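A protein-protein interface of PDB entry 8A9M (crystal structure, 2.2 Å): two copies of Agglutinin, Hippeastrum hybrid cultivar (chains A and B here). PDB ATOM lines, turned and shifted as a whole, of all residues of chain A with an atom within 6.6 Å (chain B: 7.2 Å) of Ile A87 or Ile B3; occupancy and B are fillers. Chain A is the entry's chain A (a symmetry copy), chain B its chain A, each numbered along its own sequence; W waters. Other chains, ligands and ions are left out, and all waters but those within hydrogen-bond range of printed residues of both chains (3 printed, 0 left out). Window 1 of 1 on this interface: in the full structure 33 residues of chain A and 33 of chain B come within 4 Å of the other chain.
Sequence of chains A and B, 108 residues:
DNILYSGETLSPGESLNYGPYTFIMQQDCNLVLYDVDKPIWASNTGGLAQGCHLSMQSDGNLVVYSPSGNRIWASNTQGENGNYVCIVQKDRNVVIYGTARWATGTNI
Ile A87 touches just one residue of chain B: Ile B3. Ile B3 touches just these residues of chain A: Asn A2, Ile A3 and Ile A87. Of the printed residues of chain B, Tyr A97 touches Val B85 (3.8 Å) and Tyr B97 (3.8 Å). Printed residues of chain A within 4 Å of Asn B2: Ile A3. Printed residues of chain A within 4 Å of Val B85: Tyr A97. Ser B6 touches none of the printed residues of chain A. The nearest residue of chain B that does not touch Ile A87 is Ile B87 (4.04 Å). The nearest residue of chain A that does not touch Ile B3 is Lys A90 (5.6 Å). The nearest printed residue of chain B that does not touch Val A94 is Tyr B5 (8.9 Å).
The backbone NH (N) of Ile A87 lies within hydrogen-bond range of the backbone carbonyl oxygen (O) of Val A95. O of Val A85 is in hydrogen-bond range of N of Tyr A97 (2.9 Å). The backbone carbonyl oxygen (O) of Asn A2 sits at hydrogen-bond distance from the backbone NH (N) of Val A88, 2.9 Å away. The side-chain hydroxyl (OH) of Tyr A97 lies within hydrogen-bond range of the side-chain amide nitrogen (NE2) of Gln A89 (2.6 Å). The backbone NH (N) of Tyr B5 sits at hydrogen-bond distance from the side-chain carboxylate (OE1) of Glu B8, 3.1 Å away. O of Val B85 is in hydrogen-bond range of N of Tyr B97, 2.9 Å away.
Asn A2 touches Ile B3, and with the chains exchanged Ile A3 touches Asn B2. Ile A3 touches Ile B87, and with the chains exchanged Ile A87 touches Ile B3. Val A85 touches Tyr B97, and with the chains exchanged Tyr A97 touches Val B85. Tyr B97 touches its own counterpart, Tyr A97. Positions printed for both chains: 2, 3, 4, 16, 85, 86, 87, 88 and 97. Of the 13 pairs that touch across the chains among the printed residues, 8 have their exchanged pair printed and touching as well.
The side-chain carboxylate of Glu B8 lies within salt-bridge range of the side-chain amino group of Lys A90, at 2.6 Å. OG1 of Thr B104 lies within hydrogen-bond range of OD1 of Asn A93 (3.2 Å). The backbone carbonyl oxygen (O) of Val A94 lies within hydrogen-bond range of the backbone NH (N) of Thr B104 (3.0 Å).
Ile B3 touches Asn A2 (CD1 to ND2, 3.9 Å). Asn B2 touches Ile A3. Ile B3 touches Ile A3 (CD1 to CD1, 3.9 Å). Ile B87 touches Ile A3 (CG2 to CD1, 3.8 Å). Val A85 touches Tyr B97 (CG1 to CZ, 3.8 Å). CD1 of Ile B3 touches CG2 of Ile A87, at 3.8 Å. Tyr B5 touches Gln A89. Lys A90 touches Tyr B5 (N to OH, 3.7 Å). CG1 of Val B85 touches CZ of Tyr A97 (3.8 Å). CB of Tyr A97 touches CB of Tyr B97, at 3.8 Å.
Water W2 lies within hydrogen-bond range of the backbone carbonyl oxygen of Tyr B84 (2.9 Å), the side-chain hydroxyl of Tyr A97 (3.1 Å) and the side-chain hydroxyl of Ser B6 (3.4 Å). Water W1 lies within hydrogen-bond range of OD2 of Asp B1 (3.1 Å), OD1 of Asn B2 (3.1 Å) and ND2 of Asn A2 (3.2 Å). Water W3 lies within hydrogen-bond range of the side-chain amide oxygen of Asn A2 and the side-chain amide nitrogen of Asn B2.
Hydrophobic or aromatic side chains of chain A within 4 Å of the printed part of chain B: Ile A3, Val A85, Ile A87, Val A94 and Tyr A97. Of the 17 printed residues of chain B, 8 touch a printed residue of chain A. Hydrophobic or aromatic side chains of chain B within 4 Å of the printed part of chain A: Ile B3, Tyr B5, Val B85, Ile B87 and Tyr B97. Among the printed residues, 13 pairs touch across the chains. Among the printed residues, Asp or Glu carboxylates within 4 Å of a Lys or Arg side-chain nitrogen of the other chain: Lys A90 with Glu B8 (2.6 Å).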
ATOM      1  N   ASN A   2     -13.776  -1.980 -10.134  1.00  0.00           N
ATOM      2  CA  ASN A   2     -15.208  -2.281  -9.913  1.00  0.00           C
ATOM      3  C   ASN A   2     -15.891  -2.719 -11.212  1.00  0.00           C
ATOM      4  O   ASN A   2     -17.097  -2.895 -11.171  1.00  0.00           O
ATOM      5  CB  ASN A   2     -15.930  -1.109  -9.254  1.00  0.00           C
ATOM      6  CG  ASN A   2     -16.111   0.089 -10.166  1.00  0.00           C
ATOM      7  OD1 ASN A   2     -15.257   0.384 -10.980  1.00  0.00           O
ATOM      8  ND2 ASN A   2     -17.252   0.736 -10.077  1.00  0.00           N
ATOM      9  N   ILE A   3     -15.150  -2.947 -12.295  1.00  0.00           N
ATOM     10  CA  ILE A   3     -15.714  -3.361 -13.612  1.00  0.00           C
ATOM     11  C   ILE A   3     -14.985  -4.627 -14.075  1.00  0.00           C
ATOM     12  O   ILE A   3     -13.747  -4.643 -14.059  1.00  0.00           O
ATOM     13  CB  ILE A   3     -15.570  -2.258 -14.690  1.00  0.00           C
ATOM     14  CG1 ILE A   3     -16.262  -0.951 -14.290  1.00  0.00           C
ATOM     15  CG2 ILE A   3     -16.075  -2.768 -16.035  1.00  0.00           C
ATOM     16  CD1 ILE A   3     -15.863   0.255 -15.159  1.00  0.00           C
ATOM     17  N   LEU A   4     -15.744  -5.617 -14.513  1.00  0.00           N
ATOM     18  CA  LEU A   4     -15.252  -6.794 -15.246  1.00  0.00           C
ATOM     19  C   LEU A   4     -15.780  -6.683 -16.679  1.00  0.00           C
ATOM     20  O   LEU A   4     -17.009  -6.641 -16.871  1.00  0.00           O
ATOM     21  CB  LEU A   4     -15.775  -8.051 -14.538  1.00  0.00           C
ATOM     22  CG  LEU A   4     -15.213  -9.381 -15.027  1.00  0.00           C
ATOM     23  CD1 LEU A   4     -13.718  -9.448 -14.806  1.00  0.00           C
ATOM     24  CD2 LEU A   4     -15.911 -10.520 -14.316  1.00  0.00           C
ATOM     25  N   LEU A  16     -13.964  -7.717  -7.387  1.00  0.00           N
ATOM     26  CA  LEU A  16     -14.292  -6.323  -7.759  1.00  0.00           C
ATOM     27  C   LEU A  16     -14.617  -5.584  -6.488  1.00  0.00           C
ATOM     28  O   LEU A  16     -15.231  -6.189  -5.604  1.00  0.00           O
ATOM     29  CB  LEU A  16     -15.516  -6.291  -8.661  1.00  0.00           C
ATOM     30  CG  LEU A  16     -15.412  -7.105  -9.934  1.00  0.00           C
ATOM     31  CD1 LEU A  16     -16.704  -6.954 -10.740  1.00  0.00           C
ATOM     32  CD2 LEU A  16     -14.197  -6.664 -10.740  1.00  0.00           C
ATOM     33  N   VAL A  85     -20.427  -5.378 -19.755  1.00  0.00           N
ATOM     34  CA  VAL A  85     -19.700  -5.066 -18.497  1.00  0.00           C
ATOM     35  C   VAL A  85     -20.546  -5.562 -17.338  1.00  0.00           C
ATOM     36  O   VAL A  85     -21.788  -5.466 -17.407  1.00  0.00           O
ATOM     37  CB  VAL A  85     -19.392  -3.563 -18.331  1.00  0.00           C
ATOM     38  CG1 VAL A  85     -18.272  -3.101 -19.226  1.00  0.00           C
ATOM     39  CG2 VAL A  85     -20.606  -2.699 -18.564  1.00  0.00           C
ATOM     40  N   CYS A  86     -19.859  -6.046 -16.317  1.00  0.00           N
ATOM     41  CA  CYS A  86     -20.380  -6.320 -14.972  1.00  0.00           C
ATOM     42  C   CYS A  86     -19.774  -5.302 -14.006  1.00  0.00           C
ATOM     43  O   CYS A  86     -18.560  -5.272 -13.918  1.00  0.00           O
ATOM     44  CB  CYS A  86     -20.024  -7.740 -14.555  1.00  0.00           C
ATOM     45  SG  CYS A  86     -20.677  -8.131 -12.922  1.00  0.00           S
ATOM     46  N   ILE A  87     -20.600  -4.525 -13.297  1.00  0.00           N
ATOM     47  CA  ILE A  87     -20.152  -3.364 -12.479  1.00  0.00           C
ATOM     48  C   ILE A  87     -20.644  -3.557 -11.046  1.00  0.00           C
ATOM     49  O   ILE A  87     -21.855  -3.810 -10.875  1.00  0.00           O
ATOM     50  CB  ILE A  87     -20.669  -2.025 -13.054  1.00  0.00           C
ATOM     51  CG1 ILE A  87     -20.387  -1.874 -14.546  1.00  0.00           C
ATOM     52  CG2 ILE A  87     -20.121  -0.842 -12.256  1.00  0.00           C
ATOM     53  CD1 ILE A  87     -20.909  -0.566 -15.118  1.00  0.00           C
ATOM     54  N   VAL A  88     -19.738  -3.402 -10.066  1.00  0.00           N
ATOM     55  CA  VAL A  88     -20.090  -3.123  -8.651  1.00  0.00           C
ATOM     56  C   VAL A  88     -20.251  -1.620  -8.552  1.00  0.00           C
ATOM     57  O   VAL A  88     -19.246  -0.930  -8.599  1.00  0.00           O
ATOM     58  CB  VAL A  88     -19.050  -3.632  -7.636  1.00  0.00           C
ATOM     59  CG1 VAL A  88     -19.615  -3.613  -6.216  1.00  0.00           C
ATOM     60  CG2 VAL A  88     -18.557  -5.017  -7.991  1.00  0.00           C
ATOM     61  N   GLN A  89     -21.484  -1.153  -8.458  1.00  0.00           N
ATOM     62  CA  GLN A  89     -21.848   0.276  -8.584  1.00  0.00           C
ATOM     63  C   GLN A  89     -21.684   0.970  -7.232  1.00  0.00           C
ATOM     64  O   GLN A  89     -21.707   0.273  -6.183  1.00  0.00           O
ATOM     65  CB  GLN A  89     -23.279   0.396  -9.097  1.00  0.00           C
ATOM     66  CG  GLN A  89     -23.494  -0.289 -10.443  1.00  0.00           C
ATOM     67  CD  GLN A  89     -24.840   0.045 -11.039  1.00  0.00           C
ATOM     68  OE1 GLN A  89     -25.778   0.463 -10.354  1.00  0.00           O
ATOM     69  NE2 GLN A  89     -24.940  -0.128 -12.325  1.00  0.00           N
ATOM     70  N   LYS A  90     -21.655   2.297  -7.251  1.00  0.00           N
ATOM     71  CA  LYS A  90     -21.602   3.142  -6.031  1.00  0.00           C
ATOM     72  C   LYS A  90     -22.861   2.949  -5.179  1.00  0.00           C
ATOM     73  O   LYS A  90     -22.775   3.188  -3.976  1.00  0.00           O
ATOM     74  CB  LYS A  90     -21.416   4.616  -6.386  1.00  0.00           C
ATOM     75  CG  LYS A  90     -22.446   5.181  -7.334  1.00  0.00           C
ATOM     76  CD  LYS A  90     -22.125   6.606  -7.706  1.00  0.00           C
ATOM     77  CE  LYS A  90     -23.290   7.315  -8.348  1.00  0.00           C
ATOM     78  NZ  LYS A  90     -22.824   8.571  -8.967  1.00  0.00           N
ATOM     79  N   ASN A  93     -25.418  -1.960  -5.934  1.00  0.00           N
ATOM     80  CA  ASN A  93     -25.947  -2.933  -6.911  1.00  0.00           C
ATOM     81  C   ASN A  93     -24.804  -3.490  -7.779  1.00  0.00           C
ATOM     82  O   ASN A  93     -23.846  -2.744  -8.117  1.00  0.00           O
ATOM     83  CB  ASN A  93     -27.030  -2.290  -7.764  1.00  0.00           C
ATOM     84  CG  ASN A  93     -28.109  -3.268  -8.149  1.00  0.00           C
ATOM     85  OD1 ASN A  93     -28.089  -4.416  -7.708  1.00  0.00           O
ATOM     86  ND2 ASN A  93     -29.046  -2.808  -8.959  1.00  0.00           N
ATOM     87  N   VAL A  94     -24.907  -4.758  -8.144  1.00  0.00           N
ATOM     88  CA  VAL A  94     -24.024  -5.396  -9.142  1.00  0.00           C
ATOM     89  C   VAL A  94     -24.871  -5.623 -10.376  1.00  0.00           C
ATOM     90  O   VAL A  94     -25.932  -6.271 -10.241  1.00  0.00           O
ATOM     91  CB  VAL A  94     -23.424  -6.702  -8.615  1.00  0.00           C
ATOM     92  CG1 VAL A  94     -22.515  -7.344  -9.657  1.00  0.00           C
ATOM     93  CG2 VAL A  94     -22.685  -6.483  -7.295  1.00  0.00           C
ATOM     94  N   VAL A  95     -24.443  -5.091 -11.523  1.00  0.00           N
ATOM     95  CA  VAL A  95     -25.321  -5.021 -12.728  1.00  0.00           C
ATOM     96  C   VAL A  95     -24.530  -5.445 -13.957  1.00  0.00           C
ATOM     97  O   VAL A  95     -23.377  -5.006 -14.110  1.00  0.00           O
ATOM     98  CB  VAL A  95     -25.890  -3.606 -12.917  1.00  0.00           C
ATOM     99  CG1 VAL A  95     -26.887  -3.549 -14.077  1.00  0.00           C
ATOM    100  CG2 VAL A  95     -26.511  -3.080 -11.650  1.00  0.00           C
ATOM    101  N   ILE A  96     -25.163  -6.198 -14.840  1.00  0.00           N
ATOM    102  CA  ILE A  96     -24.614  -6.485 -16.197  1.00  0.00           C
ATOM    103  C   ILE A  96     -25.295  -5.536 -17.181  1.00  0.00           C
ATOM    104  O   ILE A  96     -26.534  -5.504 -17.197  1.00  0.00           O
ATOM    105  CB  ILE A  96     -24.809  -7.968 -16.587  1.00  0.00           C
ATOM    106  CG1 ILE A  96     -24.078  -8.879 -15.601  1.00  0.00           C
ATOM    107  CG2 ILE A  96     -24.389  -8.217 -18.027  1.00  0.00           C
ATOM    108  CD1 ILE A  96     -24.394 -10.348 -15.740  1.00  0.00           C
ATOM    109  N   TYR A  97     -24.504  -4.806 -17.964  1.00  0.00           N
ATOM    110  CA  TYR A  97     -24.987  -3.915 -19.036  1.00  0.00           C
ATOM    111  C   TYR A  97     -24.389  -4.354 -20.355  1.00  0.00           C
ATOM    112  O   TYR A  97     -23.199  -4.696 -20.416  1.00  0.00           O
ATOM    113  CB  TYR A  97     -24.591  -2.451 -18.834  1.00  0.00           C
ATOM    114  CG  TYR A  97     -25.147  -1.765 -17.609  1.00  0.00           C
ATOM    115  CD1 TYR A  97     -24.463  -1.802 -16.407  1.00  0.00           C
ATOM    116  CD2 TYR A  97     -26.285  -0.987 -17.676  1.00  0.00           C
ATOM    117  CE1 TYR A  97     -24.916  -1.120 -15.292  1.00  0.00           C
ATOM    118  CE2 TYR A  97     -26.770  -0.317 -16.566  1.00  0.00           C
ATOM    119  CZ  TYR A  97     -26.072  -0.381 -15.369  1.00  0.00           C
ATOM    120  OH  TYR A  97     -26.522   0.301 -14.290  1.00  0.00           O
ATOM    121  N   ASP B   1     -15.236   9.792 -10.644  1.00  0.00           N
ATOM    122  CA  ASP B   1     -14.783   8.453 -11.079  1.00  0.00           C
ATOM    123  C   ASP B   1     -14.894   8.377 -12.614  1.00  0.00           C
ATOM    124  O   ASP B   1     -14.713   9.421 -13.280  1.00  0.00           O
ATOM    125  CB  ASP B   1     -15.589   7.365 -10.367  1.00  0.00           C
ATOM    126  CG  ASP B   1     -17.064   7.516 -10.655  1.00  0.00           C
ATOM    127  OD1 ASP B   1     -17.428   8.634 -11.133  1.00  0.00           O
ATOM    128  OD2 ASP B   1     -17.839   6.529 -10.411  1.00  0.00           O
ATOM    129  N   ASN B   2     -15.094   7.177 -13.162  1.00  0.00           N
ATOM    130  CA  ASN B   2     -14.980   6.883 -14.607  1.00  0.00           C
ATOM    131  C   ASN B   2     -16.317   6.409 -15.186  1.00  0.00           C
ATOM    132  O   ASN B   2     -16.317   6.040 -16.348  1.00  0.00           O
ATOM    133  CB  ASN B   2     -13.852   5.894 -14.890  1.00  0.00           C
ATOM    134  CG  ASN B   2     -14.143   4.483 -14.416  1.00  0.00           C
ATOM    135  OD1 ASN B   2     -14.774   4.288 -13.395  1.00  0.00           O
ATOM    136  ND2 ASN B   2     -13.743   3.501 -15.194  1.00  0.00           N
ATOM    137  N   ILE B   3     -17.414   6.476 -14.434  1.00  0.00           N
ATOM    138  CA  ILE B   3     -18.761   6.028 -14.894  1.00  0.00           C
ATOM    139  C   ILE B   3     -19.753   7.176 -14.675  1.00  0.00           C
ATOM    140  O   ILE B   3     -19.786   7.735 -13.572  1.00  0.00           O
ATOM    141  CB  ILE B   3     -19.253   4.768 -14.140  1.00  0.00           C
ATOM    142  CG1 ILE B   3     -18.300   3.579 -14.297  1.00  0.00           C
ATOM    143  CG2 ILE B   3     -20.668   4.411 -14.579  1.00  0.00           C
ATOM    144  CD1 ILE B   3     -18.568   2.432 -13.306  1.00  0.00           C
ATOM    145  N   LEU B   4     -20.554   7.461 -15.688  1.00  0.00           N
ATOM    146  CA  LEU B   4     -21.743   8.324 -15.603  1.00  0.00           C
ATOM    147  C   LEU B   4     -22.966   7.422 -15.797  1.00  0.00           C
ATOM    148  O   LEU B   4     -23.080   6.775 -16.854  1.00  0.00           O
ATOM    149  CB  LEU B   4     -21.638   9.392 -16.699  1.00  0.00           C
ATOM    150  CG  LEU B   4     -22.676  10.507 -16.653  1.00  0.00           C
ATOM    151  CD1 LEU B   4     -22.557  11.302 -15.373  1.00  0.00           C
ATOM    152  CD2 LEU B   4     -22.511  11.406 -17.860  1.00  0.00           C
ATOM    153  N   TYR B   5     -23.844   7.384 -14.824  1.00  0.00           N
ATOM    154  CA  TYR B   5     -25.064   6.553 -14.849  1.00  0.00           C
ATOM    155  C   TYR B   5     -26.166   7.350 -15.543  1.00  0.00           C
ATOM    156  O   TYR B   5     -26.204   8.602 -15.433  1.00  0.00           O
ATOM    157  CB  TYR B   5     -25.440   6.107 -13.428  1.00  0.00           C
ATOM    158  CG  TYR B   5     -24.384   5.272 -12.744  1.00  0.00           C
ATOM    159  CD1 TYR B   5     -23.341   5.857 -12.047  1.00  0.00           C
ATOM    160  CD2 TYR B   5     -24.400   3.884 -12.826  1.00  0.00           C
ATOM    161  CE1 TYR B   5     -22.362   5.088 -11.427  1.00  0.00           C
ATOM    162  CE2 TYR B   5     -23.426   3.105 -12.221  1.00  0.00           C
ATOM    163  CZ  TYR B   5     -22.408   3.705 -11.509  1.00  0.00           C
ATOM    164  OH  TYR B   5     -21.447   2.933 -10.896  1.00  0.00           O
ATOM    165  N   SER B   6     -27.077   6.654 -16.215  1.00  0.00           N
ATOM    166  CA  SER B   6     -28.279   7.284 -16.795  1.00  0.00           C
ATOM    167  C   SER B   6     -29.021   8.022 -15.674  1.00  0.00           C
ATOM    168  O   SER B   6     -29.077   7.491 -14.566  1.00  0.00           O
ATOM    169  CB  SER B   6     -29.136   6.282 -17.549  1.00  0.00           C
ATOM    170  OG  SER B   6     -29.515   5.193 -16.738  1.00  0.00           O
ATOM    171  N   GLU B   8     -27.840  11.013 -14.609  1.00  0.00           N
ATOM    172  CA  GLU B   8     -26.799  11.939 -14.067  1.00  0.00           C
ATOM    173  C   GLU B   8     -26.341  12.892 -15.171  1.00  0.00           C
ATOM    174  O   GLU B   8     -26.410  12.526 -16.350  1.00  0.00           O
ATOM    175  CB  GLU B   8     -25.572  11.195 -13.523  1.00  0.00           C
ATOM    176  CG  GLU B   8     -25.887  10.237 -12.378  1.00  0.00           C
ATOM    177  CD  GLU B   8     -24.665   9.587 -11.743  1.00  0.00           C
ATOM    178  OE1 GLU B   8     -23.647   9.388 -12.450  1.00  0.00           O
ATOM    179  OE2 GLU B   8     -24.743   9.263 -10.574  1.00  0.00           O
ATOM    180  N   LEU B  10     -22.827  15.649 -16.075  1.00  0.00           N
ATOM    181  CA  LEU B  10     -21.606  16.427 -15.786  1.00  0.00           C
ATOM    182  C   LEU B  10     -21.936  17.907 -15.972  1.00  0.00           C
ATOM    183  O   LEU B  10     -22.309  18.280 -17.100  1.00  0.00           O
ATOM    184  CB  LEU B  10     -20.492  16.038 -16.756  1.00  0.00           C
ATOM    185  CG  LEU B  10     -19.882  14.665 -16.603  1.00  0.00           C
ATOM    186  CD1 LEU B  10     -18.734  14.508 -17.574  1.00  0.00           C
ATOM    187  CD2 LEU B  10     -19.398  14.435 -15.187  1.00  0.00           C
ATOM    188  N   LEU B  16     -15.122  12.817 -16.109  1.00  0.00           N
ATOM    189  CA  LEU B  16     -14.838  11.403 -15.778  1.00  0.00           C
ATOM    190  C   LEU B  16     -13.361  11.183 -15.979  1.00  0.00           C
ATOM    191  O   LEU B  16     -12.810  11.760 -16.921  1.00  0.00           O
ATOM    192  CB  LEU B  16     -15.595  10.477 -16.717  1.00  0.00           C
ATOM    193  CG  LEU B  16     -17.098  10.658 -16.745  1.00  0.00           C
ATOM    194  CD1 LEU B  16     -17.714   9.647 -17.713  1.00  0.00           C
ATOM    195  CD2 LEU B  16     -17.670  10.508 -15.342  1.00  0.00           C
ATOM    196  N   ASN B  17     -12.762  10.376 -15.129  1.00  0.00           N
ATOM    197  CA  ASN B  17     -11.297  10.177 -15.105  1.00  0.00           C
ATOM    198  C   ASN B  17     -10.980   8.698 -14.924  1.00  0.00           C
ATOM    199  O   ASN B  17     -11.607   8.055 -14.057  1.00  0.00           O
ATOM    200  CB  ASN B  17     -10.681  11.065 -14.028  1.00  0.00           C
ATOM    201  CG  ASN B  17     -10.918  12.527 -14.329  1.00  0.00           C
ATOM    202  OD1 ASN B  17     -10.353  13.073 -15.276  1.00  0.00           O
ATOM    203  ND2 ASN B  17     -11.770  13.158 -13.555  1.00  0.00           N
ATOM    204  N   TYR B  84     -28.586   2.823 -18.420  1.00  0.00           N
ATOM    205  CA  TYR B  84     -27.388   2.826 -19.284  1.00  0.00           C
ATOM    206  C   TYR B  84     -26.221   3.336 -18.462  1.00  0.00           C
ATOM    207  O   TYR B  84     -26.453   3.987 -17.429  1.00  0.00           O
ATOM    208  CB  TYR B  84     -27.596   3.715 -20.518  1.00  0.00           C
ATOM    209  CG  TYR B  84     -28.640   3.232 -21.497  1.00  0.00           C
ATOM    210  CD1 TYR B  84     -29.975   3.510 -21.306  1.00  0.00           C
ATOM    211  CD2 TYR B  84     -28.283   2.518 -22.636  1.00  0.00           C
ATOM    212  CE1 TYR B  84     -30.939   3.089 -22.214  1.00  0.00           C
ATOM    213  CE2 TYR B  84     -29.240   2.070 -23.548  1.00  0.00           C
ATOM    214  CZ  TYR B  84     -30.570   2.376 -23.347  1.00  0.00           C
ATOM    215  OH  TYR B  84     -31.517   1.952 -24.239  1.00  0.00           O
ATOM    216  N   VAL B  85     -25.009   3.098 -18.940  1.00  0.00           N
ATOM    217  CA  VAL B  85     -23.766   3.675 -18.368  1.00  0.00           C
ATOM    218  C   VAL B  85     -22.912   4.174 -19.520  1.00  0.00           C
ATOM    219  O   VAL B  85     -22.891   3.527 -20.585  1.00  0.00           O
ATOM    220  CB  VAL B  85     -22.971   2.670 -17.507  1.00  0.00           C
ATOM    221  CG1 VAL B  85     -23.610   2.425 -16.166  1.00  0.00           C
ATOM    222  CG2 VAL B  85     -22.763   1.352 -18.211  1.00  0.00           C
ATOM    223  N   CYS B  86     -22.228   5.278 -19.266  1.00  0.00           N
ATOM    224  CA  CYS B  86     -21.122   5.816 -20.066  1.00  0.00           C
ATOM    225  C   CYS B  86     -19.829   5.655 -19.267  1.00  0.00           C
ATOM    226  O   CYS B  86     -19.776   6.196 -18.178  1.00  0.00           O
ATOM    227  CB  CYS B  86     -21.378   7.280 -20.391  1.00  0.00           C
ATOM    228  SG  CYS B  86     -20.060   7.972 -21.404  1.00  0.00           S
ATOM    229  N   ILE B  87     -18.825   4.957 -19.810  1.00  0.00           N
ATOM    230  CA  ILE B  87     -17.597   4.553 -19.071  1.00  0.00           C
ATOM    231  C   ILE B  87     -16.377   5.075 -19.826  1.00  0.00           C
ATOM    232  O   ILE B  87     -16.294   4.819 -21.046  1.00  0.00           O
ATOM    233  CB  ILE B  87     -17.513   3.020 -18.898  1.00  0.00           C
ATOM    234  CG1 ILE B  87     -18.798   2.416 -18.338  1.00  0.00           C
ATOM    235  CG2 ILE B  87     -16.297   2.632 -18.056  1.00  0.00           C
ATOM    236  CD1 ILE B  87     -18.723   0.905 -18.182  1.00  0.00           C
ATOM    237  N   VAL B  88     -15.458   5.743 -19.110  1.00  0.00           N
ATOM    238  CA  VAL B  88     -14.052   5.939 -19.546  1.00  0.00           C
ATOM    239  C   VAL B  88     -13.302   4.703 -19.097  1.00  0.00           C
ATOM    240  O   VAL B  88     -13.076   4.568 -17.905  1.00  0.00           O
ATOM    241  CB  VAL B  88     -13.396   7.215 -18.983  1.00  0.00           C
ATOM    242  CG1 VAL B  88     -12.093   7.529 -19.717  1.00  0.00           C
ATOM    243  CG2 VAL B  88     -14.336   8.398 -19.045  1.00  0.00           C
ATOM    244  N   TYR B  97     -23.016   1.585 -22.668  1.00  0.00           N
ATOM    245  CA  TYR B  97     -23.574   0.224 -22.565  1.00  0.00           C
ATOM    246  C   TYR B  97     -24.972   0.303 -21.989  1.00  0.00           C
ATOM    247  O   TYR B  97     -25.215   1.072 -21.047  1.00  0.00           O
ATOM    248  CB  TYR B  97     -22.767  -0.697 -21.648  1.00  0.00           C
ATOM    249  CG  TYR B  97     -21.348  -0.993 -22.070  1.00  0.00           C
ATOM    250  CD1 TYR B  97     -20.306  -0.177 -21.668  1.00  0.00           C
ATOM    251  CD2 TYR B  97     -21.031  -2.142 -22.767  1.00  0.00           C
ATOM    252  CE1 TYR B  97     -18.990  -0.470 -21.982  1.00  0.00           C
ATOM    253  CE2 TYR B  97     -19.725  -2.441 -23.113  1.00  0.00           C
ATOM    254  CZ  TYR B  97     -18.700  -1.599 -22.708  1.00  0.00           C
ATOM    255  OH  TYR B  97     -17.416  -1.905 -23.013  1.00  0.00           O
ATOM    256  N   THR B 104     -28.086  -7.946  -8.930  1.00  0.00           N
ATOM    257  CA  THR B 104     -28.237  -8.587  -7.616  1.00  0.00           C
ATOM    258  C   THR B 104     -29.456  -7.998  -6.905  1.00  0.00           C
ATOM    259  O   THR B 104     -30.010  -8.679  -6.080  1.00  0.00           O
ATOM    260  CB  THR B 104     -26.944  -8.450  -6.802  1.00  0.00           C
ATOM    261  OG1 THR B 104     -26.474  -7.098  -6.870  1.00  0.00           O
ATOM    262  CG2 THR B 104     -25.853  -9.379  -7.287  1.00  0.00           C
HETATM  263  O   HOH W   1     -16.527   3.739 -10.859  1.00  0.00           O
HETATM  264  O   HOH W   2     -27.587   3.123 -14.934  1.00  0.00           O
HETATM  265  O   HOH W   3     -13.159   1.089 -13.196  1.00  0.00           O
